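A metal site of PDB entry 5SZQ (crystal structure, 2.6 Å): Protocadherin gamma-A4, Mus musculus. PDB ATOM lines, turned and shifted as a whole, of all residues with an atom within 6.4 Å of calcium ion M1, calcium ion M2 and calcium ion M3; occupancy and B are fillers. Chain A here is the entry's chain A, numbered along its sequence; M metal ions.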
ATOM      1  N   GLU A 226      -4.605   6.177  21.100  1.00  0.00           N
ATOM      2  CA  GLU A 226      -4.291   5.434  22.322  1.00  0.00           C
ATOM      3  C   GLU A 226      -2.978   5.903  22.934  1.00  0.00           C
ATOM      4  O   GLU A 226      -2.972   6.540  23.990  1.00  0.00           O
ATOM      5  CB  GLU A 226      -4.221   3.938  22.048  1.00  0.00           C
ATOM      6  CG  GLU A 226      -3.845   3.126  23.273  1.00  0.00           C
ATOM      7  CD  GLU A 226      -3.937   1.650  23.029  1.00  0.00           C
ATOM      8  OE1 GLU A 226      -4.362   1.276  21.918  1.00  0.00           O
ATOM      9  OE2 GLU A 226      -3.575   0.867  23.935  1.00  0.00           O
ATOM     10  N   ASN A 227      -1.854   5.592  22.297  1.00  0.00           N
ATOM     11  CA  ASN A 227      -0.591   6.152  22.727  1.00  0.00           C
ATOM     12  C   ASN A 227      -0.482   7.556  22.167  1.00  0.00           C
ATOM     13  O   ASN A 227      -0.879   7.813  21.024  1.00  0.00           O
ATOM     14  CB  ASN A 227       0.580   5.278  22.253  1.00  0.00           C
ATOM     15  CG  ASN A 227       0.398   3.789  22.580  1.00  0.00           C
ATOM     16  OD1 ASN A 227      -0.638   3.371  23.108  1.00  0.00           O
ATOM     17  ND2 ASN A 227       1.395   2.983  22.233  1.00  0.00           N
ATOM     18  N   ASP A 284      -3.714   4.929  27.670  1.00  0.00           N
ATOM     19  CA  ASP A 284      -3.825   3.551  27.195  1.00  0.00           C
ATOM     20  C   ASP A 284      -5.301   3.175  27.087  1.00  0.00           C
ATOM     21  O   ASP A 284      -6.032   3.226  28.080  1.00  0.00           O
ATOM     22  CB  ASP A 284      -3.098   2.596  28.136  1.00  0.00           C
ATOM     23  CG  ASP A 284      -3.137   1.173  27.647  1.00  0.00           C
ATOM     24  OD1 ASP A 284      -3.296   0.964  26.430  1.00  0.00           O
ATOM     25  OD2 ASP A 284      -3.039   0.247  28.481  1.00  0.00           O
ATOM     26  N   TYR A 285      -5.724   2.782  25.883  1.00  0.00           N
ATOM     27  CA  TYR A 285      -7.151   2.523  25.659  1.00  0.00           C
ATOM     28  C   TYR A 285      -7.646   1.361  26.506  1.00  0.00           C
ATOM     29  O   TYR A 285      -8.805   1.354  26.932  1.00  0.00           O
ATOM     30  CB  TYR A 285      -7.423   2.240  24.189  1.00  0.00           C
ATOM     31  CG  TYR A 285      -8.901   2.050  23.872  1.00  0.00           C
ATOM     32  CD1 TYR A 285      -9.705   3.126  23.560  1.00  0.00           C
ATOM     33  CD2 TYR A 285      -9.487   0.793  23.910  1.00  0.00           C
ATOM     34  CE1 TYR A 285     -11.045   2.968  23.279  1.00  0.00           C
ATOM     35  CE2 TYR A 285     -10.847   0.624  23.627  1.00  0.00           C
ATOM     36  CZ  TYR A 285     -11.611   1.722  23.308  1.00  0.00           C
ATOM     37  OH  TYR A 285     -12.951   1.574  23.028  1.00  0.00           O
ATOM     38  N   GLU A 286      -6.794   0.373  26.769  1.00  0.00           N
ATOM     39  CA  GLU A 286      -7.188  -0.770  27.579  1.00  0.00           C
ATOM     40  C   GLU A 286      -7.238  -0.450  29.059  1.00  0.00           C
ATOM     41  O   GLU A 286      -7.693  -1.300  29.844  1.00  0.00           O
ATOM     42  CB  GLU A 286      -6.250  -1.943  27.327  1.00  0.00           C
ATOM     43  CG  GLU A 286      -6.412  -2.566  25.948  1.00  0.00           C
ATOM     44  CD  GLU A 286      -5.852  -1.681  24.836  1.00  0.00           C
ATOM     45  OE1 GLU A 286      -4.798  -1.053  25.060  1.00  0.00           O
ATOM     46  OE2 GLU A 286      -6.474  -1.623  23.756  1.00  0.00           O
ATOM     47  N   LEU A 316      -9.163   6.725  21.363  1.00  0.00           N
ATOM     48  CA  LEU A 316      -9.359   5.817  20.240  1.00  0.00           C
ATOM     49  C   LEU A 316      -8.438   4.613  20.397  1.00  0.00           C
ATOM     50  O   LEU A 316      -7.248   4.776  20.676  1.00  0.00           O
ATOM     51  CB  LEU A 316      -9.099   6.525  18.910  1.00  0.00           C
ATOM     52  CG  LEU A 316     -10.006   7.713  18.560  1.00  0.00           C
ATOM     53  CD1 LEU A 316      -9.527   8.410  17.303  1.00  0.00           C
ATOM     54  CD2 LEU A 316     -11.448   7.263  18.403  1.00  0.00           C
ATOM     55  N   ASP A 317      -9.002   3.423  20.221  1.00  0.00           N
ATOM     56  CA  ASP A 317      -8.239   2.185  20.361  1.00  0.00           C
ATOM     57  C   ASP A 317      -7.202   2.059  19.252  1.00  0.00           C
ATOM     58  O   ASP A 317      -7.426   2.474  18.111  1.00  0.00           O
ATOM     59  CB  ASP A 317      -9.175   0.983  20.330  1.00  0.00           C
ATOM     60  CG  ASP A 317      -8.429  -0.332  20.440  1.00  0.00           C
ATOM     61  OD1 ASP A 317      -7.551  -0.458  21.324  1.00  0.00           O
ATOM     62  OD2 ASP A 317      -8.701  -1.231  19.630  1.00  0.00           O
ATOM     63  N   GLN A 318      -6.057   1.486  19.601  1.00  0.00           N
ATOM     64  CA  GLN A 318      -4.979   1.230  18.658  1.00  0.00           C
ATOM     65  C   GLN A 318      -4.538  -0.218  18.768  1.00  0.00           C
ATOM     66  O   GLN A 318      -4.479  -0.775  19.869  1.00  0.00           O
ATOM     67  CB  GLN A 318      -3.787   2.173  18.913  1.00  0.00           C
ATOM     68  CG  GLN A 318      -2.558   1.847  18.095  1.00  0.00           C
ATOM     69  CD  GLN A 318      -1.508   2.929  18.153  1.00  0.00           C
ATOM     70  OE1 GLN A 318      -1.797   4.113  17.943  1.00  0.00           O
ATOM     71  NE2 GLN A 318      -0.268   2.539  18.436  1.00  0.00           N
ATOM     72  N   ASN A 319      -4.244  -0.831  17.618  1.00  0.00           N
ATOM     73  CA  ASN A 319      -3.742  -2.207  17.566  1.00  0.00           C
ATOM     74  C   ASN A 319      -2.300  -2.212  18.060  1.00  0.00           C
ATOM     75  O   ASN A 319      -1.337  -2.150  17.286  1.00  0.00           O
ATOM     76  CB  ASN A 319      -3.864  -2.795  16.161  1.00  0.00           C
ATOM     77  CG  ASN A 319      -3.500  -4.268  16.116  1.00  0.00           C
ATOM     78  OD1 ASN A 319      -3.435  -4.926  17.144  1.00  0.00           O
ATOM     79  ND2 ASN A 319      -3.268  -4.777  14.917  1.00  0.00           N
ATOM     80  N   ASP A 320      -2.154  -2.259  19.387  1.00  0.00           N
ATOM     81  CA  ASP A 320      -0.845  -2.259  20.041  1.00  0.00           C
ATOM     82  C   ASP A 320      -0.700  -3.448  20.984  1.00  0.00           C
ATOM     83  O   ASP A 320       0.050  -3.378  21.961  1.00  0.00           O
ATOM     84  CB  ASP A 320      -0.627  -0.951  20.790  1.00  0.00           C
ATOM     85  CG  ASP A 320      -1.486  -0.836  22.041  1.00  0.00           C
ATOM     86  OD1 ASP A 320      -2.638  -1.332  22.024  1.00  0.00           O
ATOM     87  OD2 ASP A 320      -1.005  -0.243  23.029  1.00  0.00           O
ATOM     88  N   ASN A 321      -1.405  -4.550  20.706  1.00  0.00           N
ATOM     89  CA  ASN A 321      -1.347  -5.748  21.527  1.00  0.00           C
ATOM     90  C   ASN A 321      -1.396  -6.970  20.629  1.00  0.00           C
ATOM     91  O   ASN A 321      -2.346  -7.132  19.839  1.00  0.00           O
ATOM     92  CB  ASN A 321      -2.496  -5.796  22.542  1.00  0.00           C
ATOM     93  CG  ASN A 321      -2.220  -4.959  23.768  1.00  0.00           C
ATOM     94  OD1 ASN A 321      -1.128  -5.006  24.332  1.00  0.00           O
ATOM     95  ND2 ASN A 321      -3.217  -4.171  24.183  1.00  0.00           N
ATOM     96  N   THR A 322      -0.386  -7.822  20.740  1.00  0.00           N
ATOM     97  CA  THR A 322      -0.387  -9.086  20.029  1.00  0.00           C
ATOM     98  C   THR A 322      -1.426 -10.020  20.654  1.00  0.00           C
ATOM     99  O   THR A 322      -1.702  -9.937  21.860  1.00  0.00           O
ATOM    100  CB  THR A 322       0.997  -9.737  20.100  1.00  0.00           C
ATOM    101  OG1 THR A 322       1.999  -8.769  19.761  1.00  0.00           O
ATOM    102  CG2 THR A 322       1.108 -10.915  19.140  1.00  0.00           C
ATOM    103  N   PRO A 323      -2.060 -10.875  19.864  1.00  0.00           N
ATOM    104  CA  PRO A 323      -2.935 -11.907  20.439  1.00  0.00           C
ATOM    105  C   PRO A 323      -2.167 -12.848  21.362  1.00  0.00           C
ATOM    106  O   PRO A 323      -1.010 -13.176  21.117  1.00  0.00           O
ATOM    107  CB  PRO A 323      -3.475 -12.633  19.203  1.00  0.00           C
ATOM    108  CG  PRO A 323      -3.431 -11.610  18.121  1.00  0.00           C
ATOM    109  CD  PRO A 323      -2.237 -10.752  18.406  1.00  0.00           C
ATOM    110  N   ASP A 358      -7.306 -11.238  22.725  1.00  0.00           N
ATOM    111  CA  ASP A 358      -6.591 -10.039  22.300  1.00  0.00           C
ATOM    112  C   ASP A 358      -7.060  -8.861  23.154  1.00  0.00           C
ATOM    113  O   ASP A 358      -8.263  -8.582  23.211  1.00  0.00           O
ATOM    114  CB  ASP A 358      -6.823  -9.753  20.810  1.00  0.00           C
ATOM    115  CG  ASP A 358      -5.911  -8.674  20.272  1.00  0.00           C
ATOM    116  OD1 ASP A 358      -5.192  -8.938  19.282  1.00  0.00           O
ATOM    117  OD2 ASP A 358      -5.912  -7.551  20.814  1.00  0.00           O
ATOM    118  N   LYS A 359      -6.117  -8.181  23.816  1.00  0.00           N
ATOM    119  CA  LYS A 359      -6.474  -7.121  24.759  1.00  0.00           C
ATOM    120  C   LYS A 359      -7.193  -5.955  24.076  1.00  0.00           C
ATOM    121  O   LYS A 359      -7.943  -5.229  24.739  1.00  0.00           O
ATOM    122  CB  LYS A 359      -5.235  -6.598  25.486  1.00  0.00           C
ATOM    123  CG  LYS A 359      -4.639  -7.555  26.485  1.00  0.00           C
ATOM    124  CD  LYS A 359      -3.402  -6.971  27.130  1.00  0.00           C
ATOM    125  CE  LYS A 359      -2.763  -7.971  28.083  1.00  0.00           C
ATOM    126  NZ  LYS A 359      -1.481  -7.467  28.648  1.00  0.00           N
ATOM    127  N   ASP A 360      -6.966  -5.757  22.784  1.00  0.00           N
ATOM    128  CA  ASP A 360      -7.523  -4.629  22.048  1.00  0.00           C
ATOM    129  C   ASP A 360      -9.033  -4.836  21.860  1.00  0.00           C
ATOM    130  O   ASP A 360      -9.653  -5.729  22.445  1.00  0.00           O
ATOM    131  CB  ASP A 360      -6.803  -4.458  20.720  1.00  0.00           C
ATOM    132  CG  ASP A 360      -5.287  -4.409  20.879  1.00  0.00           C
ATOM    133  OD1 ASP A 360      -4.802  -3.581  21.674  1.00  0.00           O
ATOM    134  OD2 ASP A 360      -4.585  -5.209  20.226  1.00  0.00           O
ATOM    135  N   SER A 361      -9.648  -4.000  21.017  1.00  0.00           N
ATOM    136  CA  SER A 361     -11.084  -4.039  20.800  1.00  0.00           C
ATOM    137  C   SER A 361     -11.367  -3.986  19.300  1.00  0.00           C
ATOM    138  O   SER A 361     -10.470  -3.740  18.487  1.00  0.00           O
ATOM    139  CB  SER A 361     -11.780  -2.875  21.528  1.00  0.00           C
ATOM    140  OG  SER A 361     -13.186  -3.004  21.481  1.00  0.00           O
ATOM    141  N   GLN A 363     -11.937  -4.461  15.444  1.00  0.00           N
ATOM    142  CA  GLN A 363     -11.150  -5.219  14.475  1.00  0.00           C
ATOM    143  C   GLN A 363      -9.796  -5.608  15.031  1.00  0.00           C
ATOM    144  O   GLN A 363      -9.220  -6.612  14.603  1.00  0.00           O
ATOM    145  CB  GLN A 363     -10.964  -4.427  13.185  1.00  0.00           C
ATOM    146  CG  GLN A 363     -12.189  -4.395  12.294  1.00  0.00           C
ATOM    147  CD  GLN A 363     -11.869  -3.927  10.886  1.00  0.00           C
ATOM    148  OE1 GLN A 363     -10.747  -3.536  10.598  1.00  0.00           O
ATOM    149  NE2 GLN A 363     -12.862  -3.957  10.001  1.00  0.00           N
ATOM    150  N   ASN A 364      -9.251  -4.838  15.991  1.00  0.00           N
ATOM    151  CA  ASN A 364      -7.978  -5.205  16.589  1.00  0.00           C
ATOM    152  C   ASN A 364      -8.093  -6.404  17.528  1.00  0.00           C
ATOM    153  O   ASN A 364      -7.059  -6.976  17.915  1.00  0.00           O
ATOM    154  CB  ASN A 364      -7.396  -3.992  17.322  1.00  0.00           C
ATOM    155  CG  ASN A 364      -7.406  -2.719  16.482  1.00  0.00           C
ATOM    156  OD1 ASN A 364      -7.572  -2.758  15.265  1.00  0.00           O
ATOM    157  ND2 ASN A 364      -7.220  -1.573  17.140  1.00  0.00           N
ATOM    158  N   ALA A 365      -9.317  -6.791  17.915  1.00  0.00           N
ATOM    159  CA  ALA A 365      -9.549  -7.988  18.721  1.00  0.00           C
ATOM    160  C   ALA A 365     -10.225  -9.095  17.919  1.00  0.00           C
ATOM    161  O   ALA A 365     -10.742 -10.045  18.510  1.00  0.00           O
ATOM    162  CB  ALA A 365     -10.386  -7.648  19.950  1.00  0.00           C
ATOM    163  N   LEU A 367      -9.901 -12.161  15.731  1.00  0.00           N
ATOM    164  CA  LEU A 367      -8.879 -13.173  15.510  1.00  0.00           C
ATOM    165  C   LEU A 367      -9.264 -14.118  14.380  1.00  0.00           C
ATOM    166  O   LEU A 367     -10.428 -14.509  14.244  1.00  0.00           O
ATOM    167  CB  LEU A 367      -8.634 -13.986  16.783  1.00  0.00           C
ATOM    168  CG  LEU A 367      -7.901 -13.270  17.911  1.00  0.00           C
ATOM    169  CD1 LEU A 367      -6.895 -12.284  17.342  1.00  0.00           C
ATOM    170  CD2 LEU A 367      -8.875 -12.575  18.839  1.00  0.00           C
ATOM    171  N   ASP A 411      -4.719 -10.849  14.397  1.00  0.00           N
ATOM    172  CA  ASP A 411      -5.759  -9.852  14.576  1.00  0.00           C
ATOM    173  C   ASP A 411      -6.000  -9.134  13.250  1.00  0.00           C
ATOM    174  O   ASP A 411      -5.152  -9.142  12.354  1.00  0.00           O
ATOM    175  CB  ASP A 411      -5.386  -8.865  15.681  1.00  0.00           C
ATOM    176  CG  ASP A 411      -4.076  -8.147  15.426  1.00  0.00           C
ATOM    177  OD1 ASP A 411      -3.364  -8.516  14.463  1.00  0.00           O
ATOM    178  OD2 ASP A 411      -3.754  -7.221  16.190  1.00  0.00           O
ATOM    179  N   HIS A 412      -7.181  -8.529  13.126  1.00  0.00           N
ATOM    180  CA  HIS A 412      -7.581  -7.887  11.880  1.00  0.00           C
ATOM    181  C   HIS A 412      -7.417  -6.363  11.919  1.00  0.00           C
ATOM    182  O   HIS A 412      -8.109  -5.654  11.191  1.00  0.00           O
ATOM    183  CB  HIS A 412      -9.022  -8.252  11.531  1.00  0.00           C
ATOM    184  CG  HIS A 412      -9.161  -9.641  10.974  1.00  0.00           C
ATOM    185  ND1 HIS A 412     -10.059 -10.555  11.483  1.00  0.00           N
ATOM    186  CD2 HIS A 412      -8.519 -10.258   9.960  1.00  0.00           C
ATOM    187  CE1 HIS A 412      -9.964 -11.688  10.800  1.00  0.00           C
ATOM    188  NE2 HIS A 412      -9.042 -11.527   9.866  1.00  0.00           N
ATOM    189  N   GLY A 413      -6.520  -5.867  12.760  1.00  0.00           N
ATOM    190  CA  GLY A 413      -6.253  -4.443  12.829  1.00  0.00           C
ATOM    191  C   GLY A 413      -5.228  -3.994  11.791  1.00  0.00           C
ATOM    192  O   GLY A 413      -4.774  -4.769  10.946  1.00  0.00           O
ATOM    193  N   LEU A 417      -1.111  -8.157  13.735  1.00  0.00           N
ATOM    194  CA  LEU A 417      -0.112  -8.825  14.553  1.00  0.00           C
ATOM    195  C   LEU A 417      -0.441 -10.304  14.678  1.00  0.00           C
ATOM    196  O   LEU A 417      -1.619 -10.683  14.765  1.00  0.00           O
ATOM    197  CB  LEU A 417      -0.021  -8.187  15.954  1.00  0.00           C
ATOM    198  CG  LEU A 417       0.072  -6.657  16.003  1.00  0.00           C
ATOM    199  CD1 LEU A 417      -0.064  -6.144  17.445  1.00  0.00           C
ATOM    200  CD2 LEU A 417       1.367  -6.145  15.370  1.00  0.00           C
HETATM  201 CA    CA M   1      -5.177  -0.966  22.183  1.00  0.00          CA
HETATM  202 CA    CA M   2      -1.724   0.005  25.044  1.00  0.00          CA
HETATM  203 CA    CA M   3      -4.426  -6.718  18.449  1.00  0.00          CA
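OE2 of Glu 226 lies close to N of Tyr 285 (3.5 Å).
The backbone NH (N) of Glu 226 sits at hydrogen-bond distance from the backbone carbonyl oxygen (O) of Leu 316 (3.0 Å).
The backbone carbonyl oxygen (O) of Leu 417 sits at hydrogen-bond distance from the backbone NH (N) of Asp 411, at 3.1 Å.
OD2 of Asp 317 sits at hydrogen-bond distance from ND2 of Asn 364, 2.9 Å away.
The side-chain carboxylate of Asp 317 lies within hydrogen-bond range of the backbone NH of Ser 361 (3.2 Å).
Of the 25 residues printed, 6 come within 4 Å of calcium ion M1.
The nearest printed residue that does not touch calcium ion M3 is Leu 417 (4.5 Å).
Calcium ion M1 is bound by OE2 of Glu 286 (2.1 Å), OE1 of Glu 226 (2.4 Å), O of Gln 318 (2.4 Å), OD1 of Asp 320 (2.6 Å), OD1 of Asp 317 (2.6 Å) and OD1 of Asp 360 (2.7 Å).
Calcium ion M1 has six donor atoms within binding distance.
Slightly farther from calcium ion M1 lies the side-chain carboxylate (OE1) of Glu 286 (2.9 Å).
Slightly farther from calcium ion M1 lies the side-chain carboxylate (OE2) of Glu 226 (3.0 Å).
Calcium ion M2 is bound by the side-chain carboxylate (OD2) of Asp 320 (2.2 Å), the side-chain carboxylate (OD1) of Asp 284 (2.3 Å) and the side-chain carboxylate (OE2) of Glu 226 (2.3 Å).
Calcium ion M3 is bound by the side-chain carboxylate (OD2) of Asp 360, the side-chain carboxylate (OD2) of Asp 411, the side-chain amide oxygen (OD1) of Asn 319, the side-chain carboxylate (OD1) of Asp 358, the backbone carbonyl oxygen (O) of Asn 321 and the backbone carbonyl oxygen (O) of Asn 364.
Slightly farther from calcium ion M3 lies the side-chain carboxylate (OD2) of Asp 358 (2.9 Å).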
